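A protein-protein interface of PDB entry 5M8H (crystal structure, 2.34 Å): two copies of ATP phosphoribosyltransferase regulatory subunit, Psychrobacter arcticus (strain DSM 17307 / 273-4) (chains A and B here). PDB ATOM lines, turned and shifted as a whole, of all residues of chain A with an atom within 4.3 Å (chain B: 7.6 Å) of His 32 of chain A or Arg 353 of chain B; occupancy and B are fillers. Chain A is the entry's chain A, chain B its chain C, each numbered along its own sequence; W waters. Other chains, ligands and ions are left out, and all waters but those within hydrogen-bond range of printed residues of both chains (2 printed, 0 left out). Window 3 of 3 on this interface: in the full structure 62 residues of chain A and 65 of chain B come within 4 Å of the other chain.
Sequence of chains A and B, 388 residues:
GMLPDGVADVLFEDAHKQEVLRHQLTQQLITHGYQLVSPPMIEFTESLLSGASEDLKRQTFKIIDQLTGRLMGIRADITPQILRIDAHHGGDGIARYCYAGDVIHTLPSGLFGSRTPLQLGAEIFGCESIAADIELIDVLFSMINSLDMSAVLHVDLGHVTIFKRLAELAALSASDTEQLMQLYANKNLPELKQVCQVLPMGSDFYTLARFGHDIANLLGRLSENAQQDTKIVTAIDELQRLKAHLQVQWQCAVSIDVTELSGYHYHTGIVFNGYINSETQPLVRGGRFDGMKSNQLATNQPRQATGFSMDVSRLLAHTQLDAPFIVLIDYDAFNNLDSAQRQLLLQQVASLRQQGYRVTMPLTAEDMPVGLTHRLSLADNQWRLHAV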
ATOM      1  N   GLN A  28     -30.728 -15.935 -24.514  1.00  0.00           N
ATOM      2  CA  GLN A  28     -30.707 -14.485 -24.634  1.00  0.00           C
ATOM      3  C   GLN A  28     -30.203 -13.777 -23.386  1.00  0.00           C
ATOM      4  O   GLN A  28     -29.410 -12.844 -23.492  1.00  0.00           O
ATOM      5  CB  GLN A  28     -32.093 -13.965 -24.929  1.00  0.00           C
ATOM      6  CG  GLN A  28     -32.481 -14.189 -26.355  1.00  0.00           C
ATOM      7  CD  GLN A  28     -33.625 -13.298 -26.741  1.00  0.00           C
ATOM      8  OE1 GLN A  28     -33.557 -12.014 -26.664  1.00  0.00           O
ATOM      9  NE2 GLN A  28     -34.720 -13.944 -27.154  1.00  0.00           N
ATOM     10  N   LEU A  29     -30.693 -14.197 -22.220  1.00  0.00           N
ATOM     11  CA  LEU A  29     -30.284 -13.590 -20.975  1.00  0.00           C
ATOM     12  C   LEU A  29     -28.806 -13.842 -20.743  1.00  0.00           C
ATOM     13  O   LEU A  29     -28.064 -12.931 -20.368  1.00  0.00           O
ATOM     14  CB  LEU A  29     -31.129 -14.119 -19.801  1.00  0.00           C
ATOM     15  CG  LEU A  29     -32.553 -13.529 -19.789  1.00  0.00           C
ATOM     16  CD1 LEU A  29     -33.435 -14.254 -18.789  1.00  0.00           C
ATOM     17  CD2 LEU A  29     -32.515 -12.055 -19.428  1.00  0.00           C
ATOM     18  N   ILE A  30     -28.376 -15.073 -20.989  1.00  0.00           N
ATOM     19  CA  ILE A  30     -26.976 -15.439 -20.819  1.00  0.00           C
ATOM     20  C   ILE A  30     -26.063 -14.574 -21.692  1.00  0.00           C
ATOM     21  O   ILE A  30     -25.030 -14.086 -21.194  1.00  0.00           O
ATOM     22  CB  ILE A  30     -26.759 -16.932 -21.064  1.00  0.00           C
ATOM     23  CG1 ILE A  30     -27.302 -17.725 -19.865  1.00  0.00           C
ATOM     24  CG2 ILE A  30     -25.288 -17.264 -21.249  1.00  0.00           C
ATOM     25  CD1 ILE A  30     -27.484 -19.199 -20.126  1.00  0.00           C
ATOM     26  N   THR A  31     -26.472 -14.334 -22.948  1.00  0.00           N
ATOM     27  CA  THR A  31     -25.689 -13.507 -23.860  1.00  0.00           C
ATOM     28  C   THR A  31     -25.694 -12.011 -23.527  1.00  0.00           C
ATOM     29  O   THR A  31     -24.841 -11.287 -24.026  1.00  0.00           O
ATOM     30  CB  THR A  31     -26.097 -13.696 -25.344  1.00  0.00           C
ATOM     31  OG1 THR A  31     -27.452 -13.292 -25.558  1.00  0.00           O
ATOM     32  CG2 THR A  31     -25.918 -15.152 -25.778  1.00  0.00           C
ATOM     33  N   HIS A  32     -26.633 -11.546 -22.704  1.00  0.00           N
ATOM     34  CA  HIS A  32     -26.598 -10.180 -22.155  1.00  0.00           C
ATOM     35  C   HIS A  32     -25.790 -10.063 -20.849  1.00  0.00           C
ATOM     36  O   HIS A  32     -25.773  -8.977 -20.233  1.00  0.00           O
ATOM     37  CB  HIS A  32     -28.007  -9.645 -21.938  1.00  0.00           C
ATOM     38  CG  HIS A  32     -28.699  -9.265 -23.199  1.00  0.00           C
ATOM     39  ND1 HIS A  32     -29.208 -10.198 -24.075  1.00  0.00           N
ATOM     40  CD2 HIS A  32     -28.984  -8.062 -23.734  1.00  0.00           C
ATOM     41  CE1 HIS A  32     -29.725  -9.594 -25.129  1.00  0.00           C
ATOM     42  NE2 HIS A  32     -29.649  -8.296 -24.926  1.00  0.00           N
ATOM     43  N   GLY A  33     -25.136 -11.149 -20.415  1.00  0.00           N
ATOM     44  CA  GLY A  33     -24.239 -11.094 -19.274  1.00  0.00           C
ATOM     45  C   GLY A  33     -24.846 -11.519 -17.958  1.00  0.00           C
ATOM     46  O   GLY A  33     -24.202 -11.426 -16.920  1.00  0.00           O
ATOM     47  N   TYR A  34     -26.070 -12.033 -18.001  1.00  0.00           N
ATOM     48  CA  TYR A  34     -26.740 -12.571 -16.815  1.00  0.00           C
ATOM     49  C   TYR A  34     -26.248 -14.000 -16.546  1.00  0.00           C
ATOM     50  O   TYR A  34     -26.265 -14.828 -17.437  1.00  0.00           O
ATOM     51  CB  TYR A  34     -28.268 -12.527 -16.972  1.00  0.00           C
ATOM     52  CG  TYR A  34     -28.783 -11.099 -17.022  1.00  0.00           C
ATOM     53  CD1 TYR A  34     -28.690 -10.346 -18.196  1.00  0.00           C
ATOM     54  CD2 TYR A  34     -29.314 -10.497 -15.889  1.00  0.00           C
ATOM     55  CE1 TYR A  34     -29.159  -9.052 -18.256  1.00  0.00           C
ATOM     56  CE2 TYR A  34     -29.764  -9.200 -15.923  1.00  0.00           C
ATOM     57  CZ  TYR A  34     -29.688  -8.478 -17.113  1.00  0.00           C
ATOM     58  OH  TYR A  34     -30.101  -7.182 -17.176  1.00  0.00           O
ATOM     59  N   VAL A 139     -33.569  -5.485 -21.952  1.00  0.00           N
ATOM     60  CA  VAL A 139     -33.419  -6.930 -22.067  1.00  0.00           C
ATOM     61  C   VAL A 139     -34.784  -7.596 -22.250  1.00  0.00           C
ATOM     62  O   VAL A 139     -34.976  -8.387 -23.155  1.00  0.00           O
ATOM     63  CB  VAL A 139     -32.709  -7.511 -20.828  1.00  0.00           C
ATOM     64  CG1 VAL A 139     -32.710  -9.013 -20.866  1.00  0.00           C
ATOM     65  CG2 VAL A 139     -31.239  -7.062 -20.765  1.00  0.00           C
ATOM     66  N   SER A 142     -36.279  -6.786 -25.710  1.00  0.00           N
ATOM     67  CA  SER A 142     -35.530  -7.520 -26.712  1.00  0.00           C
ATOM     68  C   SER A 142     -36.007  -8.991 -26.758  1.00  0.00           C
ATOM     69  O   SER A 142     -36.212  -9.530 -27.831  1.00  0.00           O
ATOM     70  CB  SER A 142     -34.009  -7.435 -26.462  1.00  0.00           C
ATOM     71  OG  SER A 142     -33.390  -8.730 -26.520  1.00  0.00           O
ATOM     72  N   VAL B 327     -17.487 -11.143 -22.523  1.00  0.00           N
ATOM     73  CA  VAL B 327     -17.062  -9.879 -23.110  1.00  0.00           C
ATOM     74  C   VAL B 327     -17.655  -8.689 -22.360  1.00  0.00           C
ATOM     75  O   VAL B 327     -18.850  -8.668 -22.063  1.00  0.00           O
ATOM     76  CB  VAL B 327     -17.561  -9.764 -24.553  1.00  0.00           C
ATOM     77  CG1 VAL B 327     -17.028  -8.490 -25.190  1.00  0.00           C
ATOM     78  CG2 VAL B 327     -17.193 -10.998 -25.371  1.00  0.00           C
ATOM     79  N   ILE B 329     -18.079  -4.515 -22.824  1.00  0.00           N
ATOM     80  CA  ILE B 329     -17.911  -3.340 -23.660  1.00  0.00           C
ATOM     81  C   ILE B 329     -17.256  -2.255 -22.800  1.00  0.00           C
ATOM     82  O   ILE B 329     -17.593  -2.126 -21.625  1.00  0.00           O
ATOM     83  CB  ILE B 329     -19.255  -2.892 -24.216  1.00  0.00           C
ATOM     84  CG1 ILE B 329     -19.728  -3.914 -25.239  1.00  0.00           C
ATOM     85  CG2 ILE B 329     -19.142  -1.533 -24.890  1.00  0.00           C
ATOM     86  CD1 ILE B 329     -21.229  -3.867 -25.460  1.00  0.00           C
ATOM     87  N   LEU B 346     -24.214  -1.805 -31.530  1.00  0.00           N
ATOM     88  CA  LEU B 346     -25.245  -2.699 -31.045  1.00  0.00           C
ATOM     89  C   LEU B 346     -25.519  -3.797 -32.046  1.00  0.00           C
ATOM     90  O   LEU B 346     -25.751  -4.930 -31.651  1.00  0.00           O
ATOM     91  CB  LEU B 346     -26.519  -1.918 -30.671  1.00  0.00           C
ATOM     92  CG  LEU B 346     -26.355  -1.018 -29.409  1.00  0.00           C
ATOM     93  CD1 LEU B 346     -27.576  -0.142 -29.164  1.00  0.00           C
ATOM     94  CD2 LEU B 346     -26.055  -1.821 -28.134  1.00  0.00           C
ATOM     95  N   GLN B 347     -25.459  -3.472 -33.328  1.00  0.00           N
ATOM     96  CA  GLN B 347     -25.586  -4.462 -34.406  1.00  0.00           C
ATOM     97  C   GLN B 347     -24.460  -5.491 -34.322  1.00  0.00           C
ATOM     98  O   GLN B 347     -24.687  -6.695 -34.477  1.00  0.00           O
ATOM     99  CB  GLN B 347     -25.571  -3.760 -35.766  1.00  0.00           C
ATOM    100  CG  GLN B 347     -26.923  -3.606 -36.424  1.00  0.00           C
ATOM    101  CD  GLN B 347     -26.910  -2.498 -37.470  1.00  0.00           C
ATOM    102  OE1 GLN B 347     -26.062  -2.485 -38.373  1.00  0.00           O
ATOM    103  NE2 GLN B 347     -27.826  -1.554 -37.336  1.00  0.00           N
ATOM    104  N   GLN B 348     -23.248  -5.001 -34.068  1.00  0.00           N
ATOM    105  CA  GLN B 348     -22.092  -5.858 -33.906  1.00  0.00           C
ATOM    106  C   GLN B 348     -22.212  -6.732 -32.648  1.00  0.00           C
ATOM    107  O   GLN B 348     -21.844  -7.920 -32.672  1.00  0.00           O
ATOM    108  CB  GLN B 348     -20.834  -5.002 -33.845  1.00  0.00           C
ATOM    109  CG  GLN B 348     -19.522  -5.751 -33.929  1.00  0.00           C
ATOM    110  CD  GLN B 348     -18.322  -4.849 -33.785  1.00  0.00           C
ATOM    111  OE1 GLN B 348     -18.379  -3.637 -34.055  1.00  0.00           O
ATOM    112  NE2 GLN B 348     -17.206  -5.443 -33.386  1.00  0.00           N
ATOM    113  N   VAL B 349     -22.714  -6.138 -31.558  1.00  0.00           N
ATOM    114  CA  VAL B 349     -22.902  -6.858 -30.304  1.00  0.00           C
ATOM    115  C   VAL B 349     -23.970  -7.949 -30.477  1.00  0.00           C
ATOM    116  O   VAL B 349     -23.764  -9.081 -30.055  1.00  0.00           O
ATOM    117  CB  VAL B 349     -23.257  -5.902 -29.140  1.00  0.00           C
ATOM    118  CG1 VAL B 349     -23.668  -6.682 -27.902  1.00  0.00           C
ATOM    119  CG2 VAL B 349     -22.057  -5.043 -28.773  1.00  0.00           C
ATOM    120  N   ALA B 350     -25.080  -7.601 -31.124  1.00  0.00           N
ATOM    121  CA  ALA B 350     -26.134  -8.562 -31.474  1.00  0.00           C
ATOM    122  C   ALA B 350     -25.617  -9.754 -32.258  1.00  0.00           C
ATOM    123  O   ALA B 350     -26.052 -10.878 -32.025  1.00  0.00           O
ATOM    124  CB  ALA B 350     -27.256  -7.887 -32.248  1.00  0.00           C
ATOM    125  N   SER B 351     -24.675  -9.513 -33.158  1.00  0.00           N
ATOM    126  CA  SER B 351     -24.077 -10.563 -33.972  1.00  0.00           C
ATOM    127  C   SER B 351     -23.230 -11.478 -33.099  1.00  0.00           C
ATOM    128  O   SER B 351     -23.334 -12.711 -33.192  1.00  0.00           O
ATOM    129  CB  SER B 351     -23.238  -9.946 -35.093  1.00  0.00           C
ATOM    130  OG  SER B 351     -22.783 -10.934 -35.977  1.00  0.00           O
ATOM    131  N   LEU B 352     -22.415 -10.876 -32.234  1.00  0.00           N
ATOM    132  CA  LEU B 352     -21.594 -11.651 -31.292  1.00  0.00           C
ATOM    133  C   LEU B 352     -22.461 -12.525 -30.387  1.00  0.00           C
ATOM    134  O   LEU B 352     -22.143 -13.678 -30.128  1.00  0.00           O
ATOM    135  CB  LEU B 352     -20.700 -10.727 -30.456  1.00  0.00           C
ATOM    136  CG  LEU B 352     -19.531 -10.075 -31.235  1.00  0.00           C
ATOM    137  CD1 LEU B 352     -18.822  -8.997 -30.418  1.00  0.00           C
ATOM    138  CD2 LEU B 352     -18.516 -11.124 -31.683  1.00  0.00           C
ATOM    139  N   ARG B 353     -23.560 -11.966 -29.916  1.00  0.00           N
ATOM    140  CA  ARG B 353     -24.492 -12.688 -29.045  1.00  0.00           C
ATOM    141  C   ARG B 353     -25.193 -13.842 -29.737  1.00  0.00           C
ATOM    142  O   ARG B 353     -25.442 -14.865 -29.101  1.00  0.00           O
ATOM    143  CB  ARG B 353     -25.534 -11.732 -28.474  1.00  0.00           C
ATOM    144  CG  ARG B 353     -24.972 -10.865 -27.379  1.00  0.00           C
ATOM    145  CD  ARG B 353     -26.088 -10.017 -26.835  1.00  0.00           C
ATOM    146  NE  ARG B 353     -25.642  -9.205 -25.707  1.00  0.00           N
ATOM    147  CZ  ARG B 353     -26.002  -7.942 -25.478  1.00  0.00           C
ATOM    148  NH1 ARG B 353     -26.824  -7.290 -26.295  1.00  0.00           N
ATOM    149  NH2 ARG B 353     -25.516  -7.328 -24.416  1.00  0.00           N
ATOM    150  N   GLN B 354     -25.489 -13.671 -31.029  1.00  0.00           N
ATOM    151  CA  GLN B 354     -26.051 -14.719 -31.857  1.00  0.00           C
ATOM    152  C   GLN B 354     -25.092 -15.910 -31.972  1.00  0.00           C
ATOM    153  O   GLN B 354     -25.523 -17.050 -32.045  1.00  0.00           O
ATOM    154  CB  GLN B 354     -26.363 -14.154 -33.236  1.00  0.00           C
ATOM    155  CG  GLN B 354     -26.700 -15.161 -34.310  1.00  0.00           C
ATOM    156  CD  GLN B 354     -25.555 -15.314 -35.339  1.00  0.00           C
ATOM    157  OE1 GLN B 354     -25.029 -14.305 -35.859  1.00  0.00           O
ATOM    158  NE2 GLN B 354     -25.144 -16.561 -35.602  1.00  0.00           N
ATOM    159  N   GLN B 355     -23.792 -15.629 -31.998  1.00  0.00           N
ATOM    160  CA  GLN B 355     -22.761 -16.653 -32.005  1.00  0.00           C
ATOM    161  C   GLN B 355     -22.466 -17.207 -30.613  1.00  0.00           C
ATOM    162  O   GLN B 355     -21.572 -18.041 -30.485  1.00  0.00           O
ATOM    163  CB  GLN B 355     -21.457 -16.102 -32.601  1.00  0.00           C
ATOM    164  CG  GLN B 355     -21.528 -15.685 -34.064  1.00  0.00           C
ATOM    165  CD  GLN B 355     -20.302 -14.882 -34.480  1.00  0.00           C
ATOM    166  OE1 GLN B 355     -19.150 -15.317 -34.307  1.00  0.00           O
ATOM    167  NE2 GLN B 355     -20.545 -13.677 -34.998  1.00  0.00           N
ATOM    168  N   GLY B 356     -23.153 -16.720 -29.569  1.00  0.00           N
ATOM    169  CA  GLY B 356     -22.996 -17.233 -28.204  1.00  0.00           C
ATOM    170  C   GLY B 356     -21.988 -16.549 -27.302  1.00  0.00           C
ATOM    171  O   GLY B 356     -21.687 -17.053 -26.215  1.00  0.00           O
ATOM    172  N   TYR B 357     -21.446 -15.411 -27.747  1.00  0.00           N
ATOM    173  CA  TYR B 357     -20.601 -14.561 -26.883  1.00  0.00           C
ATOM    174  C   TYR B 357     -21.469 -13.949 -25.814  1.00  0.00           C
ATOM    175  O   TYR B 357     -22.589 -13.495 -26.102  1.00  0.00           O
ATOM    176  CB  TYR B 357     -19.942 -13.440 -27.684  1.00  0.00           C
ATOM    177  CG  TYR B 357     -18.823 -13.952 -28.550  1.00  0.00           C
ATOM    178  CD1 TYR B 357     -19.078 -14.499 -29.814  1.00  0.00           C
ATOM    179  CD2 TYR B 357     -17.509 -13.928 -28.100  1.00  0.00           C
ATOM    180  CE1 TYR B 357     -18.058 -14.999 -30.594  1.00  0.00           C
ATOM    181  CE2 TYR B 357     -16.481 -14.427 -28.881  1.00  0.00           C
ATOM    182  CZ  TYR B 357     -16.765 -14.944 -30.134  1.00  0.00           C
ATOM    183  OH  TYR B 357     -15.759 -15.442 -30.905  1.00  0.00           O
ATOM    184  N   ARG B 358     -20.967 -13.930 -24.591  1.00  0.00           N
ATOM    185  CA  ARG B 358     -21.711 -13.315 -23.513  1.00  0.00           C
ATOM    186  C   ARG B 358     -21.238 -11.875 -23.333  1.00  0.00           C
ATOM    187  O   ARG B 358     -20.208 -11.629 -22.701  1.00  0.00           O
ATOM    188  CB  ARG B 358     -21.546 -14.105 -22.243  1.00  0.00           C
ATOM    189  CG  ARG B 358     -21.983 -15.535 -22.395  1.00  0.00           C
ATOM    190  CD  ARG B 358     -21.831 -16.256 -21.085  1.00  0.00           C
ATOM    191  NE  ARG B 358     -21.752 -17.697 -21.297  1.00  0.00           N
ATOM    192  CZ  ARG B 358     -21.393 -18.561 -20.361  1.00  0.00           C
ATOM    193  NH1 ARG B 358     -21.057 -18.140 -19.136  1.00  0.00           N
ATOM    194  NH2 ARG B 358     -21.381 -19.856 -20.646  1.00  0.00           N
ATOM    195  N   VAL B 359     -22.015 -10.939 -23.882  1.00  0.00           N
ATOM    196  CA  VAL B 359     -21.650  -9.538 -23.898  1.00  0.00           C
ATOM    197  C   VAL B 359     -22.434  -8.696 -22.868  1.00  0.00           C
ATOM    198  O   VAL B 359     -23.659  -8.570 -22.958  1.00  0.00           O
ATOM    199  CB  VAL B 359     -21.866  -8.928 -25.285  1.00  0.00           C
ATOM    200  CG1 VAL B 359     -21.209  -7.543 -25.358  1.00  0.00           C
ATOM    201  CG2 VAL B 359     -21.333  -9.855 -26.368  1.00  0.00           C
ATOM    202  N   THR B 360     -21.695  -8.095 -21.935  1.00  0.00           N
ATOM    203  CA  THR B 360     -22.239  -7.207 -20.921  1.00  0.00           C
ATOM    204  C   THR B 360     -22.079  -5.756 -21.388  1.00  0.00           C
ATOM    205  O   THR B 360     -20.995  -5.334 -21.805  1.00  0.00           O
ATOM    206  CB  THR B 360     -21.489  -7.382 -19.582  1.00  0.00           C
ATOM    207  OG1 THR B 360     -21.701  -8.696 -19.072  1.00  0.00           O
ATOM    208  CG2 THR B 360     -21.966  -6.396 -18.539  1.00  0.00           C
ATOM    209  N   MET B 361     -23.179  -5.010 -21.335  1.00  0.00           N
ATOM    210  CA  MET B 361     -23.192  -3.578 -21.589  1.00  0.00           C
ATOM    211  C   MET B 361     -23.108  -2.922 -20.212  1.00  0.00           C
ATOM    212  O   MET B 361     -24.065  -3.004 -19.438  1.00  0.00           O
ATOM    213  CB  MET B 361     -24.481  -3.168 -22.300  1.00  0.00           C
ATOM    214  CG  MET B 361     -24.620  -1.668 -22.534  1.00  0.00           C
ATOM    215  SD  MET B 361     -23.383  -0.956 -23.644  1.00  0.00           S
ATOM    216  CE  MET B 361     -23.796  -1.846 -25.162  1.00  0.00           C
HETATM  217  O   HOH W   1     -21.972  -9.916 -16.396  1.00  0.00           O
HETATM  218  O   HOH W   2     -25.837  -6.354 -19.763  1.00  0.00           O
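Arg 358 of chain B touches Ile 30 of chain A (NE to CG2, 3.6 Å). Tyr 357 of chain B touches Thr 31 of chain A (O to CB, 3.6 Å). Arg 358 of chain B touches Thr 31 of chain A (C to O, 3.7 Å). O of Val 359 of chain B touches N of Gly 33 of chain A, 3.9 Å away. CA of Gly 33 of chain A touches OG1 of Thr 360 of chain B (3.5 Å).
Printed residues of chain B within 4 Å of Ile 30 of chain A: Arg 358 (3.6 Å). Thr 31 of chain A touches four residues of chain B. Printed residues of chain B within 4 Å of His 32 of chain A: Arg 353 (3.3 Å) and Val 359 (3.3 Å). Arg 353 of chain B touches just these residues of chain A: Thr 31 (2.8 Å) and His 32 (3.3 Å). Gln 354 of chain B touches none of the printed residues of chain A. Of the printed residues of chain A, Tyr 357 of chain B touches Thr 31. Printed residues of chain A within 4 Å of Arg 358 of chain B: Ile 30 (3.6 Å) and Thr 31 (3.7 Å). Printed residues of chain A within 4 Å of Val 359 of chain B: Thr 31, His 32 and Gly 33. Printed residues of chain A within 4 Å of Thr 360 of chain B: Gly 33 (3.5 Å). The nearest printed residue of chain B that does not touch His 32 of chain A is Thr 360 of chain B (4.01 Å). The nearest printed residue of chain A that does not touch Thr 360 of chain B is His 32 of chain A (4.01 Å).
Of the 9 printed residues of chain A, 4 touch a printed residue of chain B. Among the printed residues, 9 pairs touch across the chains. Among the printed residues, no Asp or Glu carboxylate lies within 4 Å of a Lys or Arg side-chain nitrogen of the other chain.
Water W2 lies within hydrogen-bond range of the backbone carbonyl oxygen (O) of His 32 of chain A (2.7 Å) and the backbone NH (N) of Met 361 of chain B (3.4 Å). Water W1 lies within hydrogen-bond range of O of Gly 33 of chain A (2.7 Å) and OG1 of Thr 360 of chain B (3.0 Å).
The guanidinium group of Arg 353 of chain B lies within hydrogen-bond range of the backbone carbonyl oxygen of Val 359 of chain B, at 2.7 Å. OG1 of Thr 31 of chain A lies within hydrogen-bond range of O of Gln 28 of chain A (2.9 Å). The backbone carbonyl oxygen (O) of Gln 28 of chain A sits at hydrogen-bond distance from a ring nitrogen (ND1) of His 32 of chain A (2.7 Å). O of Val 327 of chain B lies within hydrogen-bond range of N of Thr 360 of chain B (2.9 Å). The backbone NH (N) of Val 327 of chain B sits at hydrogen-bond distance from the backbone carbonyl oxygen (O) of Arg 358 of chain B. O of Leu 352 of chain B sits at hydrogen-bond distance from N of Tyr 357 of chain B.
No position is printed for both chains. Of the 9 pairs that touch across the chains among the printed residues, none has its exchanged pair printed and touching as well.
NH1 of Arg 353 of chain B is in hydrogen-bond range of NE2 of His 32 of chain A, 3.3 Å away. O of Val 359 of chain B lies close to O of His 32 of chain A. The backbone carbonyl oxygen of Thr 31 of chain A sits at hydrogen-bond distance from the backbone NH of Val 359 of chain B (2.9 Å). The guanidinium group (NE) of Arg 353 of chain B sits at hydrogen-bond distance from the backbone carbonyl oxygen (O) of Thr 31 of chain A, at 2.8 Å.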
